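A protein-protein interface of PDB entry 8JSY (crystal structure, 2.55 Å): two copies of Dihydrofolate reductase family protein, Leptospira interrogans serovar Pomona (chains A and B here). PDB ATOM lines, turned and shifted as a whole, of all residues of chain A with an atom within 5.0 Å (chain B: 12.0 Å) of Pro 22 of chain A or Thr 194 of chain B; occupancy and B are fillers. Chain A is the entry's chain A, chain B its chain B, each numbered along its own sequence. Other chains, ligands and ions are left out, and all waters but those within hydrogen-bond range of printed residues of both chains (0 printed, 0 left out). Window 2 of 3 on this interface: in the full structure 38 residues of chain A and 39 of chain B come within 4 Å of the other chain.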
ATOM      1  N   GLY A  20     -22.229  26.387 -15.102  1.00  0.00           N
ATOM      2  CA  GLY A  20     -22.668  27.724 -14.735  1.00  0.00           C
ATOM      3  C   GLY A  20     -23.064  28.681 -15.835  1.00  0.00           C
ATOM      4  O   GLY A  20     -23.636  29.730 -15.527  1.00  0.00           O
ATOM      5  N   GLY A  21     -22.795  28.368 -17.099  1.00  0.00           N
ATOM      6  CA  GLY A  21     -23.173  29.252 -18.177  1.00  0.00           C
ATOM      7  C   GLY A  21     -22.834  28.729 -19.559  1.00  0.00           C
ATOM      8  O   GLY A  21     -21.939  27.903 -19.751  1.00  0.00           O
ATOM      9  N   PRO A  22     -23.526  29.265 -20.558  1.00  0.00           N
ATOM     10  CA  PRO A  22     -23.401  28.738 -21.929  1.00  0.00           C
ATOM     11  C   PRO A  22     -21.992  28.774 -22.524  1.00  0.00           C
ATOM     12  O   PRO A  22     -21.729  28.044 -23.487  1.00  0.00           O
ATOM     13  CB  PRO A  22     -24.337  29.647 -22.743  1.00  0.00           C
ATOM     14  CG  PRO A  22     -25.068  30.494 -21.742  1.00  0.00           C
ATOM     15  CD  PRO A  22     -24.279  30.522 -20.495  1.00  0.00           C
ATOM     16  N   GLU A  23     -21.101  29.646 -22.071  1.00  0.00           N
ATOM     17  CA  GLU A  23     -19.760  29.670 -22.645  1.00  0.00           C
ATOM     18  C   GLU A  23     -18.708  29.221 -21.642  1.00  0.00           C
ATOM     19  O   GLU A  23     -17.516  29.289 -21.937  1.00  0.00           O
ATOM     20  CB  GLU A  23     -19.412  31.061 -23.182  1.00  0.00           C
ATOM     21  CG  GLU A  23     -20.341  31.625 -24.261  1.00  0.00           C
ATOM     22  CD  GLU A  23     -19.903  33.018 -24.700  1.00  0.00           C
ATOM     23  OE1 GLU A  23     -19.696  33.874 -23.802  1.00  0.00           O
ATOM     24  OE2 GLU A  23     -19.739  33.253 -25.928  1.00  0.00           O
ATOM     25  N   GLU A  24     -19.116  28.671 -20.505  1.00  0.00           N
ATOM     26  CA  GLU A  24     -18.121  28.277 -19.475  1.00  0.00           C
ATOM     27  C   GLU A  24     -17.114  27.299 -20.088  1.00  0.00           C
ATOM     28  O   GLU A  24     -15.917  27.453 -19.810  1.00  0.00           O
ATOM     29  CB  GLU A  24     -18.808  27.689 -18.246  1.00  0.00           C
ATOM     30  CG  GLU A  24     -17.856  27.375 -17.114  1.00  0.00           C
ATOM     31  CD  GLU A  24     -18.545  26.759 -15.914  1.00  0.00           C
ATOM     32  OE1 GLU A  24     -19.711  27.092 -15.681  1.00  0.00           O
ATOM     33  OE2 GLU A  24     -17.912  25.951 -15.222  1.00  0.00           O
ATOM     34  N   THR A  26     -16.683  25.425 -24.017  1.00  0.00           N
ATOM     35  CA  THR A  26     -17.261  25.166 -25.356  1.00  0.00           C
ATOM     36  C   THR A  26     -16.547  23.978 -25.997  1.00  0.00           C
ATOM     37  O   THR A  26     -16.673  23.809 -27.211  1.00  0.00           O
ATOM     38  CB  THR A  26     -17.167  26.447 -26.191  1.00  0.00           C
ATOM     39  OG1 THR A  26     -15.795  26.828 -26.266  1.00  0.00           O
ATOM     40  CG2 THR A  26     -17.981  27.579 -25.606  1.00  0.00           C
ATOM     41  N   GLY A  33     -24.078  24.449 -21.969  1.00  0.00           N
ATOM     42  CA  GLY A  33     -23.517  25.260 -20.905  1.00  0.00           C
ATOM     43  C   GLY A  33     -24.631  25.996 -20.178  1.00  0.00           C
ATOM     44  O   GLY A  33     -25.515  26.585 -20.819  1.00  0.00           O
ATOM     45  N   GLY A  34     -24.615  25.951 -18.850  1.00  0.00           N
ATOM     46  CA  GLY A  34     -25.672  26.528 -18.047  1.00  0.00           C
ATOM     47  C   GLY A  34     -26.727  25.571 -17.507  1.00  0.00           C
ATOM     48  O   GLY A  34     -27.683  26.037 -16.870  1.00  0.00           O
ATOM     49  N   ALA A  37     -28.432  26.030 -14.188  1.00  0.00           N
ATOM     50  CA  ALA A  37     -29.108  27.287 -13.856  1.00  0.00           C
ATOM     51  C   ALA A  37     -30.570  27.113 -13.449  1.00  0.00           C
ATOM     52  O   ALA A  37     -30.945  27.623 -12.382  1.00  0.00           O
ATOM     53  CB  ALA A  37     -28.943  28.284 -15.009  1.00  0.00           C
ATOM     54  N   GLU A  40     -31.706  26.469  -9.269  1.00  0.00           N
ATOM     55  CA  GLU A  40     -31.185  27.240  -8.141  1.00  0.00           C
ATOM     56  C   GLU A  40     -32.331  27.873  -7.349  1.00  0.00           C
ATOM     57  O   GLU A  40     -33.128  28.643  -7.897  1.00  0.00           O
ATOM     58  CB  GLU A  40     -30.214  28.321  -8.622  1.00  0.00           C
ATOM     59  CG  GLU A  40     -30.699  29.101  -9.841  1.00  0.00           C
ATOM     60  CD  GLU A  40     -29.671  30.100 -10.387  1.00  0.00           C
ATOM     61  OE1 GLU A  40     -28.578  30.240  -9.797  1.00  0.00           O
ATOM     62  OE2 GLU A  40     -29.956  30.744 -11.423  1.00  0.00           O
ATOM     63  N   VAL B 190     -34.157  20.165 -21.908  1.00  0.00           N
ATOM     64  CA  VAL B 190     -33.081  20.659 -21.050  1.00  0.00           C
ATOM     65  C   VAL B 190     -33.026  22.174 -21.150  1.00  0.00           C
ATOM     66  O   VAL B 190     -32.952  22.738 -22.251  1.00  0.00           O
ATOM     67  CB  VAL B 190     -31.727  20.045 -21.448  1.00  0.00           C
ATOM     68  CG1 VAL B 190     -30.595  20.738 -20.703  1.00  0.00           C
ATOM     69  CG2 VAL B 190     -31.702  18.559 -21.159  1.00  0.00           C
ATOM     70  N   LYS B 191     -33.060  22.836 -20.002  1.00  0.00           N
ATOM     71  CA  LYS B 191     -33.020  24.286 -19.947  1.00  0.00           C
ATOM     72  C   LYS B 191     -31.677  24.738 -19.386  1.00  0.00           C
ATOM     73  O   LYS B 191     -31.137  24.119 -18.461  1.00  0.00           O
ATOM     74  CB  LYS B 191     -34.183  24.838 -19.114  1.00  0.00           C
ATOM     75  CG  LYS B 191     -35.487  25.066 -19.918  1.00  0.00           C
ATOM     76  CD  LYS B 191     -35.229  25.321 -21.429  1.00  0.00           C
ATOM     77  CE  LYS B 191     -36.485  25.830 -22.178  1.00  0.00           C
ATOM     78  NZ  LYS B 191     -37.575  24.817 -22.308  1.00  0.00           N
ATOM     79  N   THR B 192     -31.126  25.794 -19.991  1.00  0.00           N
ATOM     80  CA  THR B 192     -29.867  26.403 -19.581  1.00  0.00           C
ATOM     81  C   THR B 192     -30.077  27.893 -19.382  1.00  0.00           C
ATOM     82  O   THR B 192     -30.778  28.538 -20.170  1.00  0.00           O
ATOM     83  CB  THR B 192     -28.755  26.211 -20.633  1.00  0.00           C
ATOM     84  OG1 THR B 192     -29.191  26.749 -21.890  1.00  0.00           O
ATOM     85  CG2 THR B 192     -28.387  24.743 -20.803  1.00  0.00           C
ATOM     86  N   GLY B 193     -29.453  28.439 -18.341  1.00  0.00           N
ATOM     87  CA  GLY B 193     -29.433  29.864 -18.107  1.00  0.00           C
ATOM     88  C   GLY B 193     -28.008  30.351 -17.921  1.00  0.00           C
ATOM     89  O   GLY B 193     -27.063  29.815 -18.515  1.00  0.00           O
ATOM     90  N   THR B 194     -27.866  31.391 -17.089  1.00  0.00           N
ATOM     91  CA  THR B 194     -26.564  31.865 -16.626  1.00  0.00           C
ATOM     92  C   THR B 194     -26.646  32.075 -15.122  1.00  0.00           C
ATOM     93  O   THR B 194     -27.436  32.897 -14.651  1.00  0.00           O
ATOM     94  CB  THR B 194     -26.137  33.163 -17.333  1.00  0.00           C
ATOM     95  OG1 THR B 194     -25.760  32.898 -18.696  1.00  0.00           O
ATOM     96  CG2 THR B 194     -24.957  33.792 -16.617  1.00  0.00           C
ATOM     97  N   VAL B 195     -25.850  31.330 -14.367  1.00  0.00           N
ATOM     98  CA  VAL B 195     -25.829  31.510 -12.926  1.00  0.00           C
ATOM     99  C   VAL B 195     -25.310  32.905 -12.600  1.00  0.00           C
ATOM    100  O   VAL B 195     -24.128  33.193 -12.792  1.00  0.00           O
ATOM    101  CB  VAL B 195     -24.969  30.447 -12.238  1.00  0.00           C
ATOM    102  CG1 VAL B 195     -24.654  30.870 -10.812  1.00  0.00           C
ATOM    103  CG2 VAL B 195     -25.675  29.120 -12.261  1.00  0.00           C
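Of chain B, only Thr 194 (3.8 Å) and Val 195 (3.0 Å) come within 4 Å of Gly 20 of chain A.
Pro 22 of chain A touches just these residues of chain B: Gly 193 (3.5 Å) and Thr 194 (3.3 Å).
No residue of chain B comes within 4 Å of Glu 23 of chain A.
No residue of chain B comes within 4 Å of Thr 26 of chain A.
Of the printed residues of chain B, Ala 37 of chain A touches Gly 193 (3.4 Å) and Thr 194 (3.9 Å).
Of the printed residues of chain B, Glu 40 of chain A touches Val 195 (3.97 Å).
Lys 191 of chain B touches none of the printed residues of chain A.
Of the printed residues of chain A, Thr 192 of chain B touches Gly 33 (3.3 Å) and Gly 34 (3.5 Å).
Printed residues of chain A within 4 Å of Gly 193 of chain B: Gly 21 (3.9 Å), Pro 22 (3.5 Å), Gly 34 (3.3 Å) and Ala 37 (3.4 Å).
Printed residues of chain A within 4 Å of Val 195 of chain B: Gly 20 and Glu 40.
No position is printed for both chains.
Hydrophobic or aromatic side chains of chain B that line the printed part of chain A: Val 195.
Printed residues of chain A that touch a printed residue of chain B: Gly 20, Gly 21, Pro 22, Gly 33, Gly 34, Ala 37 and Glu 40.
Among the printed residues, no Asp or Glu carboxylate lies within 4 Å of a Lys or Arg side-chain nitrogen of the other chain.
The backbone carbonyl oxygen of Gly 21 of chain A sits close to the backbone NH of Gly 34 of chain A (3.4 Å).
N of Gly 20 of chain A is in hydrogen-bond range of OE1 of Glu 24 of chain A (2.7 Å).
The backbone carbonyl oxygen of Gly 20 of chain A is in hydrogen-bond range of the backbone NH of Val 195 of chain B, at 3.0 Å.
O of Gly 34 of chain A lies within hydrogen-bond range of N of Gly 193 of chain B (3.3 Å).
Among the printed residues, merely in contact across the chains: Gly 33 of chain A with Thr 192 of chain B (3.3 Å), Pro 22 of chain A with Thr 194 of chain B (3.3 Å), Ala 37 of chain A with Gly 193 of chain B (3.4 Å), Pro 22 of chain A with Gly 193 of chain B (3.5 Å), Gly 34 of chain A with Thr 192 of chain B (3.5 Å), Gly 20 of chain A with Thr 194 of chain B (3.8 Å), Ala 37 of chain A with Thr 194 of chain B (3.9 Å), Gly 21 of chain A with Gly 193 of chain B (3.9 Å) and Glu 40 of chain A with Val 195 of chain B (3.97 Å).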
